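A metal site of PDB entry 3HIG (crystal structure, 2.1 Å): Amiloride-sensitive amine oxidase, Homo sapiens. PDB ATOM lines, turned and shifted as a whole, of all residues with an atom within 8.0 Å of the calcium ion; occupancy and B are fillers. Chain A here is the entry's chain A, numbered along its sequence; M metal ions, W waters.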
ATOM      1  N   GLU A 542     -11.958 -16.614   3.234  1.00  0.00           N
ATOM      2  CA  GLU A 542     -12.354 -15.680   4.287  1.00  0.00           C
ATOM      3  C   GLU A 542     -11.451 -14.469   4.379  1.00  0.00           C
ATOM      4  O   GLU A 542     -11.936 -13.348   4.520  1.00  0.00           O
ATOM      5  CB  GLU A 542     -12.396 -16.374   5.653  1.00  0.00           C
ATOM      6  CG  GLU A 542     -13.501 -17.405   5.801  1.00  0.00           C
ATOM      7  CD  GLU A 542     -13.412 -18.157   7.114  1.00  0.00           C
ATOM      8  OE1 GLU A 542     -12.286 -18.560   7.489  1.00  0.00           O
ATOM      9  OE2 GLU A 542     -14.462 -18.325   7.781  1.00  0.00           O
ATOM     10  N   ARG A 543     -10.134 -14.683   4.305  1.00  0.00           N
ATOM     11  CA  ARG A 543      -9.162 -13.597   4.477  1.00  0.00           C
ATOM     12  C   ARG A 543      -9.327 -12.503   3.429  1.00  0.00           C
ATOM     13  O   ARG A 543      -9.100 -11.323   3.717  1.00  0.00           O
ATOM     14  CB  ARG A 543      -7.724 -14.115   4.417  1.00  0.00           C
ATOM     15  CG  ARG A 543      -7.300 -14.939   5.612  1.00  0.00           C
ATOM     16  CD  ARG A 543      -7.084 -14.116   6.863  1.00  0.00           C
ATOM     17  NE  ARG A 543      -6.309 -14.861   7.875  1.00  0.00           N
ATOM     18  CZ  ARG A 543      -5.986 -14.380   9.079  1.00  0.00           C
ATOM     19  NH1 ARG A 543      -6.369 -13.174   9.460  1.00  0.00           N
ATOM     20  NH2 ARG A 543      -5.271 -15.128   9.929  1.00  0.00           N
ATOM     21  N   VAL A 604     -16.287 -11.623   6.739  1.00  0.00           N
ATOM     22  CA  VAL A 604     -17.203 -12.703   6.340  1.00  0.00           C
ATOM     23  C   VAL A 604     -16.622 -14.022   6.801  1.00  0.00           C
ATOM     24  O   VAL A 604     -15.449 -14.298   6.548  1.00  0.00           O
ATOM     25  CB  VAL A 604     -17.427 -12.680   4.821  1.00  0.00           C
ATOM     26  CG1 VAL A 604     -18.390 -13.818   4.388  1.00  0.00           C
ATOM     27  CG2 VAL A 604     -18.008 -11.329   4.414  1.00  0.00           C
ATOM     28  N   THR A 605     -17.409 -14.825   7.531  1.00  0.00           N
ATOM     29  CA  THR A 605     -16.945 -16.133   7.977  1.00  0.00           C
ATOM     30  C   THR A 605     -17.875 -17.229   7.498  1.00  0.00           C
ATOM     31  O   THR A 605     -19.054 -16.978   7.165  1.00  0.00           O
ATOM     32  CB  THR A 605     -16.788 -16.230   9.526  1.00  0.00           C
ATOM     33  OG1 THR A 605     -18.054 -16.046  10.171  1.00  0.00           O
ATOM     34  CG2 THR A 605     -15.776 -15.189  10.014  1.00  0.00           C
ATOM     35  N   LYS A 606     -17.349 -18.436   7.455  1.00  0.00           N
ATOM     36  CA  LYS A 606     -18.173 -19.636   7.274  1.00  0.00           C
ATOM     37  C   LYS A 606     -18.900 -19.982   8.577  1.00  0.00           C
ATOM     38  O   LYS A 606     -18.291 -20.006   9.653  1.00  0.00           O
ATOM     39  CB  LYS A 606     -17.324 -20.795   6.785  1.00  0.00           C
ATOM     40  CG  LYS A 606     -18.037 -22.142   6.755  1.00  0.00           C
ATOM     41  CD  LYS A 606     -17.191 -23.164   5.999  1.00  0.00           C
ATOM     42  CE  LYS A 606     -17.787 -24.534   6.085  1.00  0.00           C
ATOM     43  NZ  LYS A 606     -17.194 -25.336   4.989  1.00  0.00           N
ATOM     44  N   TYR A 607     -20.206 -20.227   8.473  1.00  0.00           N
ATOM     45  CA  TYR A 607     -21.066 -20.576   9.620  1.00  0.00           C
ATOM     46  C   TYR A 607     -20.531 -21.792  10.395  1.00  0.00           C
ATOM     47  O   TYR A 607     -20.110 -22.789   9.794  1.00  0.00           O
ATOM     48  CB  TYR A 607     -22.497 -20.877   9.191  1.00  0.00           C
ATOM     49  CG  TYR A 607     -23.396 -21.195  10.359  1.00  0.00           C
ATOM     50  CD1 TYR A 607     -23.504 -22.477  10.878  1.00  0.00           C
ATOM     51  CD2 TYR A 607     -24.141 -20.190  10.978  1.00  0.00           C
ATOM     52  CE1 TYR A 607     -24.321 -22.755  11.990  1.00  0.00           C
ATOM     53  CE2 TYR A 607     -24.959 -20.457  12.070  1.00  0.00           C
ATOM     54  CZ  TYR A 607     -25.047 -21.725  12.566  1.00  0.00           C
ATOM     55  OH  TYR A 607     -25.861 -21.961  13.639  1.00  0.00           O
ATOM     56  N   ARG A 608     -20.622 -21.704  11.713  1.00  0.00           N
ATOM     57  CA  ARG A 608     -20.207 -22.804  12.562  1.00  0.00           C
ATOM     58  C   ARG A 608     -20.870 -22.597  13.930  1.00  0.00           C
ATOM     59  O   ARG A 608     -20.871 -21.479  14.458  1.00  0.00           O
ATOM     60  CB  ARG A 608     -18.659 -22.803  12.627  1.00  0.00           C
ATOM     61  CG  ARG A 608     -18.013 -23.729  13.572  1.00  0.00           C
ATOM     62  CD  ARG A 608     -16.511 -23.879  13.258  1.00  0.00           C
ATOM     63  NE  ARG A 608     -16.371 -24.490  11.955  1.00  0.00           N
ATOM     64  CZ  ARG A 608     -15.860 -23.918  10.868  1.00  0.00           C
ATOM     65  NH1 ARG A 608     -15.356 -22.689  10.874  1.00  0.00           N
ATOM     66  NH2 ARG A 608     -15.848 -24.609   9.752  1.00  0.00           N
ATOM     67  N   GLU A 611     -19.060 -20.894  16.660  1.00  0.00           N
ATOM     68  CA  GLU A 611     -18.681 -19.472  16.450  1.00  0.00           C
ATOM     69  C   GLU A 611     -19.906 -18.566  16.367  1.00  0.00           C
ATOM     70  O   GLU A 611     -19.986 -17.675  15.512  1.00  0.00           O
ATOM     71  CB  GLU A 611     -17.872 -19.325  15.147  1.00  0.00           C
ATOM     72  CG  GLU A 611     -16.580 -20.176  15.085  1.00  0.00           C
ATOM     73  CD  GLU A 611     -15.851 -20.059  13.746  1.00  0.00           C
ATOM     74  OE1 GLU A 611     -16.303 -19.291  12.861  1.00  0.00           O
ATOM     75  OE2 GLU A 611     -14.839 -20.778  13.560  1.00  0.00           O
ATOM     76  N   PHE A 630     -12.261 -13.083  18.145  1.00  0.00           N
ATOM     77  CA  PHE A 630     -12.872 -13.088  16.821  1.00  0.00           C
ATOM     78  C   PHE A 630     -11.874 -13.401  15.691  1.00  0.00           C
ATOM     79  O   PHE A 630     -12.216 -14.086  14.733  1.00  0.00           O
ATOM     80  CB  PHE A 630     -13.587 -11.752  16.544  1.00  0.00           C
ATOM     81  CG  PHE A 630     -14.200 -11.704  15.193  1.00  0.00           C
ATOM     82  CD1 PHE A 630     -15.434 -12.281  14.980  1.00  0.00           C
ATOM     83  CD2 PHE A 630     -13.518 -11.140  14.120  1.00  0.00           C
ATOM     84  CE1 PHE A 630     -16.000 -12.247  13.710  1.00  0.00           C
ATOM     85  CE2 PHE A 630     -14.080 -11.097  12.861  1.00  0.00           C
ATOM     86  CZ  PHE A 630     -15.320 -11.661  12.649  1.00  0.00           C
ATOM     87  N   GLU A 631     -10.660 -12.849  15.805  1.00  0.00           N
ATOM     88  CA  GLU A 631      -9.581 -13.062  14.808  1.00  0.00           C
ATOM     89  C   GLU A 631      -9.355 -14.556  14.513  1.00  0.00           C
ATOM     90  O   GLU A 631      -9.026 -14.931  13.370  1.00  0.00           O
ATOM     91  CB  GLU A 631      -8.272 -12.426  15.317  1.00  0.00           C
ATOM     92  CG  GLU A 631      -7.069 -12.549  14.381  1.00  0.00           C
ATOM     93  CD  GLU A 631      -7.212 -11.740  13.084  1.00  0.00           C
ATOM     94  OE1 GLU A 631      -8.050 -10.798  13.022  1.00  0.00           O
ATOM     95  OE2 GLU A 631      -6.461 -12.047  12.120  1.00  0.00           O
ATOM     96  N   GLN A 632      -9.561 -15.389  15.526  1.00  0.00           N
ATOM     97  CA  GLN A 632      -9.385 -16.819  15.348  1.00  0.00           C
ATOM     98  C   GLN A 632     -10.364 -17.440  14.369  1.00  0.00           C
ATOM     99  O   GLN A 632     -10.018 -18.467  13.752  1.00  0.00           O
ATOM    100  CB  GLN A 632      -9.419 -17.578  16.688  1.00  0.00           C
ATOM    101  CG  GLN A 632      -8.187 -17.276  17.539  1.00  0.00           C
ATOM    102  CD  GLN A 632      -8.250 -17.852  18.949  1.00  0.00           C
ATOM    103  OE1 GLN A 632      -9.179 -18.591  19.315  1.00  0.00           O
ATOM    104  NE2 GLN A 632      -7.253 -17.484  19.763  1.00  0.00           N
ATOM    105  N   PHE A 633     -11.541 -16.848  14.182  1.00  0.00           N
ATOM    106  CA  PHE A 633     -12.504 -17.359  13.187  1.00  0.00           C
ATOM    107  C   PHE A 633     -11.951 -17.212  11.744  1.00  0.00           C
ATOM    108  O   PHE A 633     -12.403 -17.909  10.830  1.00  0.00           O
ATOM    109  CB  PHE A 633     -13.869 -16.644  13.234  1.00  0.00           C
ATOM    110  CG  PHE A 633     -14.567 -16.624  14.586  1.00  0.00           C
ATOM    111  CD1 PHE A 633     -14.147 -17.374  15.674  1.00  0.00           C
ATOM    112  CD2 PHE A 633     -15.717 -15.835  14.735  1.00  0.00           C
ATOM    113  CE1 PHE A 633     -14.851 -17.331  16.886  1.00  0.00           C
ATOM    114  CE2 PHE A 633     -16.416 -15.783  15.905  1.00  0.00           C
ATOM    115  CZ  PHE A 633     -15.985 -16.525  16.992  1.00  0.00           C
ATOM    116  N   LEU A 634     -10.999 -16.305  11.549  1.00  0.00           N
ATOM    117  CA  LEU A 634     -10.358 -16.069  10.237  1.00  0.00           C
ATOM    118  C   LEU A 634      -9.072 -16.876  10.057  1.00  0.00           C
ATOM    119  O   LEU A 634      -8.597 -16.990   8.952  1.00  0.00           O
ATOM    120  CB  LEU A 634     -10.041 -14.588  10.055  1.00  0.00           C
ATOM    121  CG  LEU A 634     -11.181 -13.605  10.287  1.00  0.00           C
ATOM    122  CD1 LEU A 634     -10.715 -12.125  10.195  1.00  0.00           C
ATOM    123  CD2 LEU A 634     -12.278 -13.881   9.254  1.00  0.00           C
ATOM    124  N   HIS A 635      -8.531 -17.441  11.122  1.00  0.00           N
ATOM    125  CA  HIS A 635      -7.287 -18.205  11.025  1.00  0.00           C
ATOM    126  C   HIS A 635      -7.298 -19.295   9.968  1.00  0.00           C
ATOM    127  O   HIS A 635      -6.331 -19.447   9.236  1.00  0.00           O
ATOM    128  CB  HIS A 635      -6.893 -18.815  12.385  1.00  0.00           C
ATOM    129  CG  HIS A 635      -6.315 -17.832  13.353  1.00  0.00           C
ATOM    130  ND1 HIS A 635      -6.016 -18.165  14.660  1.00  0.00           N
ATOM    131  CD2 HIS A 635      -5.996 -16.528  13.209  1.00  0.00           C
ATOM    132  CE1 HIS A 635      -5.500 -17.099  15.268  1.00  0.00           C
ATOM    133  NE2 HIS A 635      -5.475 -16.092  14.408  1.00  0.00           N
ATOM    134  N   ASN A 636      -8.364 -20.065   9.880  1.00  0.00           N
ATOM    135  CA  ASN A 636      -8.340 -21.176   8.947  1.00  0.00           C
ATOM    136  C   ASN A 636      -8.675 -20.779   7.509  1.00  0.00           C
ATOM    137  O   ASN A 636      -8.684 -21.643   6.641  1.00  0.00           O
ATOM    138  CB  ASN A 636      -9.198 -22.351   9.411  1.00  0.00           C
ATOM    139  CG  ASN A 636     -10.623 -21.953   9.757  1.00  0.00           C
ATOM    140  OD1 ASN A 636     -11.063 -20.831   9.499  1.00  0.00           O
ATOM    141  ND2 ASN A 636     -11.338 -22.869  10.382  1.00  0.00           N
ATOM    142  N   ASN A 637      -8.961 -19.503   7.268  1.00  0.00           N
ATOM    143  CA  ASN A 637      -9.095 -18.987   5.908  1.00  0.00           C
ATOM    144  C   ASN A 637      -9.886 -19.921   5.010  1.00  0.00           C
ATOM    145  O   ASN A 637      -9.427 -20.353   3.947  1.00  0.00           O
ATOM    146  CB  ASN A 637      -7.703 -18.646   5.312  1.00  0.00           C
ATOM    147  CG  ASN A 637      -7.800 -17.778   4.049  1.00  0.00           C
ATOM    148  OD1 ASN A 637      -8.805 -17.120   3.840  1.00  0.00           O
ATOM    149  ND2 ASN A 637      -6.753 -17.806   3.195  1.00  0.00           N
ATOM    150  N   GLU A 638     -11.109 -20.194   5.430  1.00  0.00           N
ATOM    151  CA  GLU A 638     -11.923 -21.164   4.750  1.00  0.00           C
ATOM    152  C   GLU A 638     -12.491 -20.672   3.430  1.00  0.00           C
ATOM    153  O   GLU A 638     -12.659 -19.460   3.222  1.00  0.00           O
ATOM    154  CB  GLU A 638     -13.059 -21.580   5.665  1.00  0.00           C
ATOM    155  CG  GLU A 638     -12.551 -22.324   6.847  1.00  0.00           C
ATOM    156  CD  GLU A 638     -13.630 -22.620   7.860  1.00  0.00           C
ATOM    157  OE1 GLU A 638     -13.957 -21.735   8.679  1.00  0.00           O
ATOM    158  OE2 GLU A 638     -14.115 -23.772   7.845  1.00  0.00           O
ATOM    159  N   ASN A 639     -12.781 -21.623   2.556  1.00  0.00           N
ATOM    160  CA  ASN A 639     -13.426 -21.338   1.290  1.00  0.00           C
ATOM    161  C   ASN A 639     -14.845 -20.827   1.529  1.00  0.00           C
ATOM    162  O   ASN A 639     -15.584 -21.415   2.295  1.00  0.00           O
ATOM    163  CB  ASN A 639     -13.445 -22.572   0.409  1.00  0.00           C
ATOM    164  CG  ASN A 639     -13.833 -22.255  -1.023  1.00  0.00           C
ATOM    165  OD1 ASN A 639     -15.003 -22.121  -1.315  1.00  0.00           O
ATOM    166  ND2 ASN A 639     -12.835 -22.092  -1.905  1.00  0.00           N
ATOM    167  N   ILE A 640     -15.186 -19.698   0.912  1.00  0.00           N
ATOM    168  CA  ILE A 640     -16.504 -19.080   1.095  1.00  0.00           C
ATOM    169  C   ILE A 640     -17.294 -18.941  -0.211  1.00  0.00           C
ATOM    170  O   ILE A 640     -18.164 -18.073  -0.322  1.00  0.00           O
ATOM    171  CB  ILE A 640     -16.421 -17.707   1.808  1.00  0.00           C
ATOM    172  CG1 ILE A 640     -15.469 -16.763   1.072  1.00  0.00           C
ATOM    173  CG2 ILE A 640     -15.988 -17.892   3.322  1.00  0.00           C
ATOM    174  CD1 ILE A 640     -15.723 -15.303   1.381  1.00  0.00           C
HETATM  175 CA    CA M   1     -13.246 -19.709   9.566  1.00  0.00          CA
HETATM  176  O   HOH W   1     -13.062 -20.733  11.743  1.00  0.00           O
HETATM  177  O   HOH W   2     -15.494 -19.676  10.424  1.00  0.00           O
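Merely in contact with the calcium ion: Arg 608 (3.9 Å).
Five residues have an atom within 4 Å of the calcium ion: Glu 542, Arg 608, Phe 633, Asn 636 and Glu 638.
The calcium ion is bound by the side-chain carboxylate (OE1) of Glu 638, the backbone carbonyl oxygen (O) of Phe 633, water W2, water W1, the side-chain amide oxygen (OD1) of Asn 636, the side-chain carboxylate (OE1) of Glu 542 and the side-chain carboxylate (OE2) of Glu 542.
The side-chain carboxylate of Glu 611 lies within salt-bridge range of the guanidinium group of Arg 608 (3.3 Å).
OE2 of Glu 542 lies close to N of Lys 606 (2.9 Å).
The backbone NH (N) of Glu 542 sits at hydrogen-bond distance from the side-chain amide oxygen (OD1) of Asn 637, 3.3 Å away.
The guanidinium group of Arg 608 lies within salt-bridge range of the side-chain carboxylate of Glu 638 (2.7 Å).
Water W1 lies within hydrogen-bond range of OE2 of Glu 611, ND2 of Asn 636 and NH1 of Arg 608.
Water W2 lies within hydrogen-bond range of the side-chain carboxylate (OE1) of Glu 611 (2.6 Å), the backbone carbonyl oxygen (O) of Lys 606 (2.9 Å) and the guanidinium group (NH1) of Arg 608 (3.0 Å).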
